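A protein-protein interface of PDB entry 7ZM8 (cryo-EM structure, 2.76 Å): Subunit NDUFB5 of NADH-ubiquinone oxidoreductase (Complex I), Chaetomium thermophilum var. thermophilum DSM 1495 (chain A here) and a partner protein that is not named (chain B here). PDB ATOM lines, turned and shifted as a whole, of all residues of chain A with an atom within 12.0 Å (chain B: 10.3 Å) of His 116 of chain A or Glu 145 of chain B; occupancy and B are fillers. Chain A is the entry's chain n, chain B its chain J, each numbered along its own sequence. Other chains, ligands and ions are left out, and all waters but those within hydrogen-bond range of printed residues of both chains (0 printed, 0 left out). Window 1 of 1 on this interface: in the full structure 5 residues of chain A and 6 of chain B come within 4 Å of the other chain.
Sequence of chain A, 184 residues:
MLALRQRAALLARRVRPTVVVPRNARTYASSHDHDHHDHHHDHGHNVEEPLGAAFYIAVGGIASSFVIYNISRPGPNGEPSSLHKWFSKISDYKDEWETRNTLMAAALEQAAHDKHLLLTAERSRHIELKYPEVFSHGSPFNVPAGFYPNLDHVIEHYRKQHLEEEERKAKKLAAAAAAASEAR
NE2 of His 113 of chain A sits at hydrogen-bond distance from OH of Tyr 141 of chain B (2.9 Å). ND1 of His 113 of chain A is in hydrogen-bond range of OE1 of Glu 145 of chain B, at 3.2 Å. A ring nitrogen (ND1) of His 116 of chain A sits at hydrogen-bond distance from the side-chain carboxylate (OE2) of Glu 145 of chain B (3.1 Å). NH2 of Arg 148 of chain B is in salt-bridge range of OE1 of Glu 109 of chain A (3.3 Å). NH1 of Arg 151 of chain B is in salt-bridge range of OE1 of Glu 109 of chain A (3.6 Å).
OD1 of Asp 139 of chain B lies close to N of Tyr 141 of chain B (3.4 Å). The side-chain carboxylate of Glu 145 of chain B is in salt-bridge range of the guanidinium group of Arg 148 of chain B. The side-chain carboxylate (OE1) of Glu 145 of chain B lies within salt-bridge range of the side-chain amino group (NZ) of Lys 149 of chain B. The guanidinium group (NE) of Arg 151 of chain B lies within hydrogen-bond range of the backbone carbonyl oxygen (O) of Arg 148 of chain B (3.4 Å). OG1 of Thr 120 of chain A is in hydrogen-bond range of O of His 116 of chain A (2.6 Å).
Among the printed residues, pairs that only touch across the chains: His 113 of chain A with Arg 148 of chain B (3.6 Å), His 116 of chain A with Lys 144 of chain B (3.8 Å), Leu 117 of chain A with Tyr 141 of chain B (3.6 Å), Thr 120 of chain A with Glu 140 of chain B (3.9 Å) and Thr 120 of chain A with Tyr 141 of chain B (3.5 Å).
Of the printed residues of chain B, Glu 109 of chain A touches Arg 148 and Arg 151. Ala 112 of chain A touches none of the printed residues of chain B. His 113 of chain A touches just these residues of chain B: Tyr 141, Glu 145 and Arg 148. Lys 115 of chain A touches none of the printed residues of chain B. Of chain B, only Lys 144 (3.8 Å) and Glu 145 (3.1 Å) come within 4 Å of His 116 of chain A. Leu 118 of chain A touches none of the printed residues of chain B. Of the printed residues of chain A, Glu 140 of chain B touches Thr 120 (3.9 Å). Of chain A, only His 113 (2.9 Å), Leu 117 (3.6 Å) and Thr 120 (3.5 Å) come within 4 Å of Tyr 141 of chain B. No residue of chain A comes within 4 Å of Glu 142 of chain B. Of chain A, only His 116 comes within 4 Å of Lys 144 of chain B. Glu 145 of chain B touches two residues of chain A. Arg 148 of chain B touches just these residues of chain A: Glu 109 (3.3 Å) and His 113 (3.6 Å). No residue of chain A comes within 4 Å of Lys 149 of chain B. Of the printed residues of chain A, Arg 151 of chain B touches Glu 109 (3.6 Å). The nearest residue of chain A that does not touch Glu 145 of chain B is Ala 112 of chain A (4.8 Å). The nearest printed residue of chain B that does not touch Glu 109 of chain A is Lys 149 of chain B (6.6 Å).
Of the 18 printed residues of chain A, 5 touch a printed residue of chain B. Printed residues of chain A that touch a printed residue of chain B: Glu 109, His 113, His 116, Leu 117 and Thr 120. Of the 15 printed residues of chain B, 6 touch a printed residue of chain A. Printed residues of chain B that touch a printed residue of chain A: Glu 140, Tyr 141, Lys 144, Glu 145, Arg 148 and Arg 151. Among the printed residues, 10 pairs touch across the chains. Among the printed residues, Asp or Glu carboxylates within 4 Å of a Lys or Arg side-chain nitrogen of the other chain: Glu 109 of chain A with Arg 148 of chain B (3.3 Å) and Glu 109 of chain A with Arg 151 of chain B (3.6 Å).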
ATOM      1  N   ALA A 106       9.025   4.898   4.439  1.00  0.00           N
ATOM      2  CA  ALA A 106       9.561   6.062   5.131  1.00  0.00           C
ATOM      3  C   ALA A 106       9.694   7.259   4.198  1.00  0.00           C
ATOM      4  O   ALA A 106       9.343   8.384   4.569  1.00  0.00           O
ATOM      5  CB  ALA A 106      10.911   5.715   5.753  1.00  0.00           C
ATOM      6  N   ALA A 107      10.144   7.070   2.964  1.00  0.00           N
ATOM      7  CA  ALA A 107      10.358   8.176   2.005  1.00  0.00           C
ATOM      8  C   ALA A 107       9.028   8.728   1.514  1.00  0.00           C
ATOM      9  O   ALA A 107       8.869   9.947   1.472  1.00  0.00           O
ATOM     10  CB  ALA A 107      11.166   7.667   0.856  1.00  0.00           C
ATOM     11  N   LEU A 108       8.118   7.845   1.115  1.00  0.00           N
ATOM     12  CA  LEU A 108       6.808   8.285   0.576  1.00  0.00           C
ATOM     13  C   LEU A 108       6.018   8.953   1.696  1.00  0.00           C
ATOM     14  O   LEU A 108       5.162   9.792   1.374  1.00  0.00           O
ATOM     15  CB  LEU A 108       6.103   7.089  -0.065  1.00  0.00           C
ATOM     16  CG  LEU A 108       6.586   6.795  -1.483  1.00  0.00           C
ATOM     17  CD1 LEU A 108       6.588   5.309  -1.781  1.00  0.00           C
ATOM     18  CD2 LEU A 108       5.763   7.558  -2.503  1.00  0.00           C
ATOM     19  N   GLU A 109       6.296   8.602   2.952  1.00  0.00           N
ATOM     20  CA  GLU A 109       5.688   9.330   4.089  1.00  0.00           C
ATOM     21  C   GLU A 109       6.318  10.718   4.193  1.00  0.00           C
ATOM     22  O   GLU A 109       5.575  11.668   4.505  1.00  0.00           O
ATOM     23  CB  GLU A 109       5.981   8.596   5.388  1.00  0.00           C
ATOM     24  CG  GLU A 109       5.051   7.433   5.668  1.00  0.00           C
ATOM     25  CD  GLU A 109       3.713   7.829   6.266  1.00  0.00           C
ATOM     26  OE1 GLU A 109       3.530   9.025   6.562  1.00  0.00           O
ATOM     27  OE2 GLU A 109       2.858   6.939   6.431  1.00  0.00           O
ATOM     28  N   GLN A 110       7.620  10.849   3.962  1.00  0.00           N
ATOM     29  CA  GLN A 110       8.288  12.172   4.013  1.00  0.00           C
ATOM     30  C   GLN A 110       7.718  13.063   2.913  1.00  0.00           C
ATOM     31  O   GLN A 110       7.419  14.223   3.195  1.00  0.00           O
ATOM     32  CB  GLN A 110       9.801  12.046   3.888  1.00  0.00           C
ATOM     33  CG  GLN A 110      10.535  13.376   3.972  1.00  0.00           C
ATOM     34  CD  GLN A 110      10.372  14.045   5.314  1.00  0.00           C
ATOM     35  OE1 GLN A 110      10.158  15.252   5.406  1.00  0.00           O
ATOM     36  NE2 GLN A 110      10.466  13.259   6.374  1.00  0.00           N
ATOM     37  N   ALA A 111       7.626  12.550   1.692  1.00  0.00           N
ATOM     38  CA  ALA A 111       7.163  13.341   0.541  1.00  0.00           C
ATOM     39  C   ALA A 111       5.740  13.840   0.765  1.00  0.00           C
ATOM     40  O   ALA A 111       5.429  14.916   0.253  1.00  0.00           O
ATOM     41  CB  ALA A 111       7.284  12.487  -0.683  1.00  0.00           C
ATOM     42  N   ALA A 112       4.892  13.066   1.432  1.00  0.00           N
ATOM     43  CA  ALA A 112       3.524  13.519   1.769  1.00  0.00           C
ATOM     44  C   ALA A 112       3.576  14.760   2.669  1.00  0.00           C
ATOM     45  O   ALA A 112       2.758  15.653   2.463  1.00  0.00           O
ATOM     46  CB  ALA A 112       2.829  12.397   2.482  1.00  0.00           C
ATOM     47  N   HIS A 113       4.480  14.780   3.646  1.00  0.00           N
ATOM     48  CA  HIS A 113       4.662  15.927   4.560  1.00  0.00           C
ATOM     49  C   HIS A 113       5.142  17.096   3.715  1.00  0.00           C
ATOM     50  O   HIS A 113       4.659  18.220   3.937  1.00  0.00           O
ATOM     51  CB  HIS A 113       5.708  15.532   5.607  1.00  0.00           C
ATOM     52  CG  HIS A 113       6.100  16.594   6.572  1.00  0.00           C
ATOM     53  ND1 HIS A 113       5.793  16.504   7.909  1.00  0.00           N
ATOM     54  CD2 HIS A 113       6.811  17.731   6.418  1.00  0.00           C
ATOM     55  CE1 HIS A 113       6.280  17.550   8.540  1.00  0.00           C
ATOM     56  NE2 HIS A 113       6.908  18.320   7.645  1.00  0.00           N
ATOM     57  N   ASP A 114       6.051  16.835   2.778  1.00  0.00           N
ATOM     58  CA  ASP A 114       6.632  17.901   1.920  1.00  0.00           C
ATOM     59  C   ASP A 114       5.551  18.466   1.003  1.00  0.00           C
ATOM     60  O   ASP A 114       5.511  19.687   0.860  1.00  0.00           O
ATOM     61  CB  ASP A 114       7.903  17.418   1.230  1.00  0.00           C
ATOM     62  CG  ASP A 114       9.024  17.140   2.210  1.00  0.00           C
ATOM     63  OD1 ASP A 114       8.810  17.375   3.413  1.00  0.00           O
ATOM     64  OD2 ASP A 114      10.099  16.699   1.763  1.00  0.00           O
ATOM     65  N   LYS A 115       4.764  17.601   0.366  1.00  0.00           N
ATOM     66  CA  LYS A 115       3.693  18.032  -0.568  1.00  0.00           C
ATOM     67  C   LYS A 115       2.724  18.920   0.190  1.00  0.00           C
ATOM     68  O   LYS A 115       2.249  19.890  -0.398  1.00  0.00           O
ATOM     69  CB  LYS A 115       2.952  16.822  -1.140  1.00  0.00           C
ATOM     70  CG  LYS A 115       1.613  17.102  -1.808  1.00  0.00           C
ATOM     71  CD  LYS A 115       0.925  15.851  -2.297  1.00  0.00           C
ATOM     72  CE  LYS A 115      -0.539  16.054  -2.623  1.00  0.00           C
ATOM     73  NZ  LYS A 115      -1.186  14.788  -3.042  1.00  0.00           N
ATOM     74  N   HIS A 116       2.516  18.638   1.473  1.00  0.00           N
ATOM     75  CA  HIS A 116       1.562  19.418   2.291  1.00  0.00           C
ATOM     76  C   HIS A 116       2.231  20.750   2.629  1.00  0.00           C
ATOM     77  O   HIS A 116       1.555  21.752   2.587  1.00  0.00           O
ATOM     78  CB  HIS A 116       1.231  18.630   3.561  1.00  0.00           C
ATOM     79  CG  HIS A 116       0.038  17.743   3.464  1.00  0.00           C
ATOM     80  ND1 HIS A 116      -0.400  16.992   4.533  1.00  0.00           N
ATOM     81  CD2 HIS A 116      -0.813  17.488   2.451  1.00  0.00           C
ATOM     82  CE1 HIS A 116      -1.468  16.311   4.183  1.00  0.00           C
ATOM     83  NE2 HIS A 116      -1.741  16.598   2.914  1.00  0.00           N
ATOM     84  N   LEU A 117       3.537  20.746   2.898  1.00  0.00           N
ATOM     85  CA  LEU A 117       4.246  22.001   3.272  1.00  0.00           C
ATOM     86  C   LEU A 117       4.285  22.976   2.095  1.00  0.00           C
ATOM     87  O   LEU A 117       3.979  24.148   2.295  1.00  0.00           O
ATOM     88  CB  LEU A 117       5.658  21.627   3.729  1.00  0.00           C
ATOM     89  CG  LEU A 117       6.536  22.775   4.218  1.00  0.00           C
ATOM     90  CD1 LEU A 117       6.095  23.239   5.596  1.00  0.00           C
ATOM     91  CD2 LEU A 117       7.993  22.352   4.237  1.00  0.00           C
ATOM     92  N   LEU A 118       4.610  22.486   0.901  1.00  0.00           N
ATOM     93  CA  LEU A 118       4.735  23.364  -0.287  1.00  0.00           C
ATOM     94  C   LEU A 118       3.358  23.823  -0.772  1.00  0.00           C
ATOM     95  O   LEU A 118       3.264  24.966  -1.233  1.00  0.00           O
ATOM     96  CB  LEU A 118       5.477  22.596  -1.381  1.00  0.00           C
ATOM     97  CG  LEU A 118       6.969  22.368  -1.160  1.00  0.00           C
ATOM     98  CD1 LEU A 118       7.460  21.207  -2.010  1.00  0.00           C
ATOM     99  CD2 LEU A 118       7.762  23.624  -1.472  1.00  0.00           C
ATOM    100  N   LEU A 119       2.333  22.980  -0.657  1.00  0.00           N
ATOM    101  CA  LEU A 119       0.997  23.313  -1.223  1.00  0.00           C
ATOM    102  C   LEU A 119       0.141  24.127  -0.248  1.00  0.00           C
ATOM    103  O   LEU A 119      -0.917  24.607  -0.681  1.00  0.00           O
ATOM    104  CB  LEU A 119       0.296  22.006  -1.607  1.00  0.00           C
ATOM    105  CG  LEU A 119      -0.182  21.883  -3.050  1.00  0.00           C
ATOM    106  CD1 LEU A 119       0.912  22.286  -4.021  1.00  0.00           C
ATOM    107  CD2 LEU A 119      -0.641  20.464  -3.330  1.00  0.00           C
ATOM    108  N   THR A 120       0.550  24.250   1.014  1.00  0.00           N
ATOM    109  CA  THR A 120      -0.299  24.951   2.014  1.00  0.00           C
ATOM    110  C   THR A 120       0.503  26.105   2.593  1.00  0.00           C
ATOM    111  O   THR A 120       0.387  26.345   3.805  1.00  0.00           O
ATOM    112  CB  THR A 120      -0.781  24.035   3.148  1.00  0.00           C
ATOM    113  OG1 THR A 120       0.341  23.598   3.914  1.00  0.00           O
ATOM    114  CG2 THR A 120      -1.590  22.849   2.673  1.00  0.00           C
ATOM    115  N   ALA A 121       1.238  26.822   1.746  1.00  0.00           N
ATOM    116  CA  ALA A 121       2.135  27.861   2.263  1.00  0.00           C
ATOM    117  C   ALA A 121       1.454  29.224   2.262  1.00  0.00           C
ATOM    118  O   ALA A 121       0.518  29.411   1.492  1.00  0.00           O
ATOM    119  CB  ALA A 121       3.433  27.818   1.500  1.00  0.00           C
ATOM    120  N   GLU A 122       1.899  30.116   3.143  1.00  0.00           N
ATOM    121  CA  GLU A 122       1.260  31.444   3.261  1.00  0.00           C
ATOM    122  C   GLU A 122       1.444  32.217   1.954  1.00  0.00           C
ATOM    123  O   GLU A 122       2.560  32.272   1.453  1.00  0.00           O
ATOM    124  CB  GLU A 122       1.853  32.182   4.460  1.00  0.00           C
ATOM    125  CG  GLU A 122       1.206  33.526   4.739  1.00  0.00           C
ATOM    126  CD  GLU A 122      -0.201  33.464   5.308  1.00  0.00           C
ATOM    127  OE1 GLU A 122      -0.588  32.393   5.818  1.00  0.00           O
ATOM    128  OE2 GLU A 122      -0.907  34.489   5.243  1.00  0.00           O
ATOM    129  N   ARG A 123       0.368  32.794   1.439  1.00  0.00           N
ATOM    130  CA  ARG A 123       0.446  33.626   0.221  1.00  0.00           C
ATOM    131  C   ARG A 123       0.941  34.984   0.689  1.00  0.00           C
ATOM    132  O   ARG A 123       0.566  35.390   1.795  1.00  0.00           O
ATOM    133  CB  ARG A 123      -0.963  33.774  -0.366  1.00  0.00           C
ATOM    134  CG  ARG A 123      -1.059  34.481  -1.705  1.00  0.00           C
ATOM    135  CD  ARG A 123      -2.515  34.817  -1.949  1.00  0.00           C
ATOM    136  NE  ARG A 123      -2.791  35.138  -3.339  1.00  0.00           N
ATOM    137  CZ  ARG A 123      -3.425  34.332  -4.177  1.00  0.00           C
ATOM    138  NH1 ARG A 123      -3.873  33.163  -3.759  1.00  0.00           N
ATOM    139  NH2 ARG A 123      -3.624  34.706  -5.425  1.00  0.00           N
ATOM    140  N   VAL B 138      -7.934  29.658   8.919  1.00  0.00           N
ATOM    141  CA  VAL B 138      -7.197  28.842   9.933  1.00  0.00           C
ATOM    142  C   VAL B 138      -5.844  28.457   9.319  1.00  0.00           C
ATOM    143  O   VAL B 138      -5.562  28.923   8.198  1.00  0.00           O
ATOM    144  CB  VAL B 138      -8.027  27.604  10.328  1.00  0.00           C
ATOM    145  CG1 VAL B 138      -8.033  26.534   9.246  1.00  0.00           C
ATOM    146  CG2 VAL B 138      -7.628  27.026  11.677  1.00  0.00           C
ATOM    147  N   ASP B 139      -5.038  27.644  10.014  1.00  0.00           N
ATOM    148  CA  ASP B 139      -3.757  27.167   9.429  1.00  0.00           C
ATOM    149  C   ASP B 139      -4.037  25.922   8.595  1.00  0.00           C
ATOM    150  O   ASP B 139      -4.421  24.914   9.179  1.00  0.00           O
ATOM    151  CB  ASP B 139      -2.729  26.848  10.515  1.00  0.00           C
ATOM    152  CG  ASP B 139      -1.365  26.477   9.961  1.00  0.00           C
ATOM    153  OD1 ASP B 139      -1.088  26.830   8.800  1.00  0.00           O
ATOM    154  OD2 ASP B 139      -0.592  25.841  10.696  1.00  0.00           O
ATOM    155  N   GLU B 140      -3.833  26.009   7.284  1.00  0.00           N
ATOM    156  CA  GLU B 140      -4.055  24.855   6.377  1.00  0.00           C
ATOM    157  C   GLU B 140      -3.074  23.727   6.682  1.00  0.00           C
ATOM    158  O   GLU B 140      -3.493  22.583   6.631  1.00  0.00           O
ATOM    159  CB  GLU B 140      -4.007  25.287   4.913  1.00  0.00           C
ATOM    160  CG  GLU B 140      -5.359  25.715   4.375  1.00  0.00           C
ATOM    161  CD  GLU B 140      -6.409  24.616   4.341  1.00  0.00           C
ATOM    162  OE1 GLU B 140      -6.028  23.436   4.209  1.00  0.00           O
ATOM    163  OE2 GLU B 140      -7.607  24.943   4.452  1.00  0.00           O
ATOM    164  N   TYR B 141      -1.824  24.056   6.979  1.00  0.00           N
ATOM    165  CA  TYR B 141      -0.794  23.025   7.254  1.00  0.00           C
ATOM    166  C   TYR B 141      -1.172  22.242   8.501  1.00  0.00           C
ATOM    167  O   TYR B 141      -1.088  21.016   8.483  1.00  0.00           O
ATOM    168  CB  TYR B 141       0.578  23.671   7.410  1.00  0.00           C
ATOM    169  CG  TYR B 141       1.723  22.736   7.683  1.00  0.00           C
ATOM    170  CD1 TYR B 141       2.338  22.040   6.659  1.00  0.00           C
ATOM    171  CD2 TYR B 141       2.201  22.564   8.968  1.00  0.00           C
ATOM    172  CE1 TYR B 141       3.396  21.186   6.906  1.00  0.00           C
ATOM    173  CE2 TYR B 141       3.264  21.723   9.233  1.00  0.00           C
ATOM    174  CZ  TYR B 141       3.860  21.031   8.197  1.00  0.00           C
ATOM    175  OH  TYR B 141       4.904  20.202   8.463  1.00  0.00           O
ATOM    176  N   GLU B 142      -1.621  22.944   9.533  1.00  0.00           N
ATOM    177  CA  GLU B 142      -2.061  22.265  10.772  1.00  0.00           C
ATOM    178  C   GLU B 142      -3.282  21.394  10.464  1.00  0.00           C
ATOM    179  O   GLU B 142      -3.308  20.251  10.937  1.00  0.00           O
ATOM    180  CB  GLU B 142      -2.334  23.314  11.849  1.00  0.00           C
ATOM    181  CG  GLU B 142      -2.507  22.728  13.237  1.00  0.00           C
ATOM    182  CD  GLU B 142      -1.249  22.125  13.838  1.00  0.00           C
ATOM    183  OE1 GLU B 142      -0.147  22.615  13.521  1.00  0.00           O
ATOM    184  OE2 GLU B 142      -1.375  21.161  14.618  1.00  0.00           O
ATOM    185  N   ARG B 143      -4.240  21.909   9.694  1.00  0.00           N
ATOM    186  CA  ARG B 143      -5.496  21.161   9.422  1.00  0.00           C
ATOM    187  C   ARG B 143      -5.205  19.897   8.619  1.00  0.00           C
ATOM    188  O   ARG B 143      -5.736  18.843   8.980  1.00  0.00           O
ATOM    189  CB  ARG B 143      -6.468  22.057   8.657  1.00  0.00           C
ATOM    190  CG  ARG B 143      -7.779  21.381   8.284  1.00  0.00           C
ATOM    191  CD  ARG B 143      -8.375  21.949   7.011  1.00  0.00           C
ATOM    192  NE  ARG B 143      -9.637  21.307   6.676  1.00  0.00           N
ATOM    193  CZ  ARG B 143     -10.832  21.764   7.030  1.00  0.00           C
ATOM    194  NH1 ARG B 143     -11.923  21.106   6.681  1.00  0.00           N
ATOM    195  NH2 ARG B 143     -10.934  22.881   7.729  1.00  0.00           N
ATOM    196  N   LYS B 144      -4.377  20.013   7.580  1.00  0.00           N
ATOM    197  CA  LYS B 144      -4.064  18.869   6.692  1.00  0.00           C
ATOM    198  C   LYS B 144      -3.239  17.849   7.456  1.00  0.00           C
ATOM    199  O   LYS B 144      -3.510  16.651   7.324  1.00  0.00           O
ATOM    200  CB  LYS B 144      -3.376  19.381   5.427  1.00  0.00           C
ATOM    201  CG  LYS B 144      -4.210  20.293   4.540  1.00  0.00           C
ATOM    202  CD  LYS B 144      -5.547  19.702   4.157  1.00  0.00           C
ATOM    203  CE  LYS B 144      -5.431  18.478   3.277  1.00  0.00           C
ATOM    204  NZ  LYS B 144      -6.758  17.885   2.990  1.00  0.00           N
ATOM    205  N   GLU B 145      -2.269  18.325   8.225  1.00  0.00           N
ATOM    206  CA  GLU B 145      -1.363  17.417   8.970  1.00  0.00           C
ATOM    207  C   GLU B 145      -2.132  16.661  10.058  1.00  0.00           C
ATOM    208  O   GLU B 145      -1.837  15.481  10.264  1.00  0.00           O
ATOM    209  CB  GLU B 145      -0.112  18.171   9.415  1.00  0.00           C
ATOM    210  CG  GLU B 145       0.865  18.437   8.290  1.00  0.00           C
ATOM    211  CD  GLU B 145       1.758  17.263   7.933  1.00  0.00           C
ATOM    212  OE1 GLU B 145       2.748  17.050   8.645  1.00  0.00           O
ATOM    213  OE2 GLU B 145       1.459  16.568   6.947  1.00  0.00           O
ATOM    214  N   PHE B 146      -3.100  17.301  10.706  1.00  0.00           N
ATOM    215  CA  PHE B 146      -3.915  16.637  11.746  1.00  0.00           C
ATOM    216  C   PHE B 146      -4.687  15.502  11.111  1.00  0.00           C
ATOM    217  O   PHE B 146      -4.816  14.443  11.715  1.00  0.00           O
ATOM    218  CB  PHE B 146      -4.964  17.592  12.311  1.00  0.00           C
ATOM    219  CG  PHE B 146      -5.874  16.957  13.329  1.00  0.00           C
ATOM    220  CD1 PHE B 146      -5.405  16.623  14.587  1.00  0.00           C
ATOM    221  CD2 PHE B 146      -7.195  16.675  13.023  1.00  0.00           C
ATOM    222  CE1 PHE B 146      -6.238  16.024  15.518  1.00  0.00           C
ATOM    223  CE2 PHE B 146      -8.025  16.072  13.952  1.00  0.00           C
ATOM    224  CZ  PHE B 146      -7.546  15.751  15.199  1.00  0.00           C
ATOM    225  N   LEU B 147      -5.201  15.748   9.920  1.00  0.00           N
ATOM    226  CA  LEU B 147      -5.997  14.729   9.223  1.00  0.00           C
ATOM    227  C   LEU B 147      -5.112  13.543   8.856  1.00  0.00           C
ATOM    228  O   LEU B 147      -5.609  12.428   8.941  1.00  0.00           O
ATOM    229  CB  LEU B 147      -6.631  15.405   8.016  1.00  0.00           C
ATOM    230  CG  LEU B 147      -7.781  16.359   8.315  1.00  0.00           C
ATOM    231  CD1 LEU B 147      -8.254  17.031   7.037  1.00  0.00           C
ATOM    232  CD2 LEU B 147      -8.924  15.627   8.993  1.00  0.00           C
ATOM    233  N   ARG B 148      -3.852  13.769   8.492  1.00  0.00           N
ATOM    234  CA  ARG B 148      -2.957  12.674   8.028  1.00  0.00           C
ATOM    235  C   ARG B 148      -2.398  11.891   9.220  1.00  0.00           C
ATOM    236  O   ARG B 148      -2.159  10.687   9.072  1.00  0.00           O
ATOM    237  CB  ARG B 148      -1.781  13.265   7.244  1.00  0.00           C
ATOM    238  CG  ARG B 148      -0.744  12.237   6.811  1.00  0.00           C
ATOM    239  CD  ARG B 148       0.492  12.803   6.144  1.00  0.00           C
ATOM    240  NE  ARG B 148       1.273  13.675   7.001  1.00  0.00           N
ATOM    241  CZ  ARG B 148       2.396  13.327   7.604  1.00  0.00           C
ATOM    242  NH1 ARG B 148       3.030  14.199   8.365  1.00  0.00           N
ATOM    243  NH2 ARG B 148       2.894  12.118   7.435  1.00  0.00           N
ATOM    244  N   LYS B 149      -2.228  12.535  10.367  1.00  0.00           N
ATOM    245  CA  LYS B 149      -1.654  11.876  11.528  1.00  0.00           C
ATOM    246  C   LYS B 149      -2.683  11.526  12.594  1.00  0.00           C
ATOM    247  O   LYS B 149      -2.305  11.064  13.673  1.00  0.00           O
ATOM    248  CB  LYS B 149      -0.546  12.744  12.117  1.00  0.00           C
ATOM    249  CG  LYS B 149       0.705  12.757  11.266  1.00  0.00           C
ATOM    250  CD  LYS B 149       1.695  13.791  11.752  1.00  0.00           C
ATOM    251  CE  LYS B 149       1.286  15.185  11.327  1.00  0.00           C
ATOM    252  NZ  LYS B 149       2.280  16.209  11.740  1.00  0.00           N
ATOM    253  N   ASN B 150      -3.972  11.717  12.317  1.00  0.00           N
ATOM    254  CA  ASN B 150      -5.031  11.292  13.237  1.00  0.00           C
ATOM    255  C   ASN B 150      -5.359   9.825  12.972  1.00  0.00           C
ATOM    256  O   ASN B 150      -6.448   9.455  12.536  1.00  0.00           O
ATOM    257  CB  ASN B 150      -6.258  12.179  13.087  1.00  0.00           C
ATOM    258  CG  ASN B 150      -7.329  11.863  14.101  1.00  0.00           C
ATOM    259  OD1 ASN B 150      -7.043  11.351  15.181  1.00  0.00           O
ATOM    260  ND2 ASN B 150      -8.574  12.166  13.759  1.00  0.00           N
ATOM    261  N   ARG B 151      -4.369   8.981  13.243  1.00  0.00           N
ATOM    262  CA  ARG B 151      -4.464   7.576  12.876  1.00  0.00           C
ATOM    263  C   ARG B 151      -5.361   6.791  13.825  1.00  0.00           C
ATOM    264  O   ARG B 151      -6.083   5.891  13.388  1.00  0.00           O
ATOM    265  CB  ARG B 151      -3.063   6.974  12.813  1.00  0.00           C
ATOM    266  CG  ARG B 151      -2.106   7.816  12.015  1.00  0.00           C
ATOM    267  CD  ARG B 151      -1.284   6.976  11.059  1.00  0.00           C
ATOM    268  NE  ARG B 151      -0.626   7.782  10.033  1.00  0.00           N
ATOM    269  CZ  ARG B 151       0.517   8.437  10.208  1.00  0.00           C
ATOM    270  NH1 ARG B 151       1.038   9.136   9.214  1.00  0.00           N
ATOM    271  NH2 ARG B 151       1.136   8.403  11.375  1.00  0.00           N
ATOM    272  N   ARG B 153      -8.319   6.733  17.022  1.00  0.00           N
ATOM    273  CA  ARG B 153      -9.379   7.595  17.584  1.00  0.00           C
ATOM    274  C   ARG B 153      -9.904   6.967  18.859  1.00  0.00           C
ATOM    275  O   ARG B 153      -9.663   5.792  19.065  1.00  0.00           O
ATOM    276  CB  ARG B 153     -10.517   7.751  16.571  1.00  0.00           C
ATOM    277  CG  ARG B 153     -10.285   8.811  15.506  1.00  0.00           C
ATOM    278  CD  ARG B 153     -11.434   8.792  14.520  1.00  0.00           C
ATOM    279  NE  ARG B 153     -11.410   9.882  13.558  1.00  0.00           N
ATOM    280  CZ  ARG B 153     -10.751   9.855  12.408  1.00  0.00           C
ATOM    281  NH1 ARG B 153     -10.043   8.793  12.075  1.00  0.00           N
ATOM    282  NH2 ARG B 153     -10.788  10.898  11.602  1.00  0.00           N
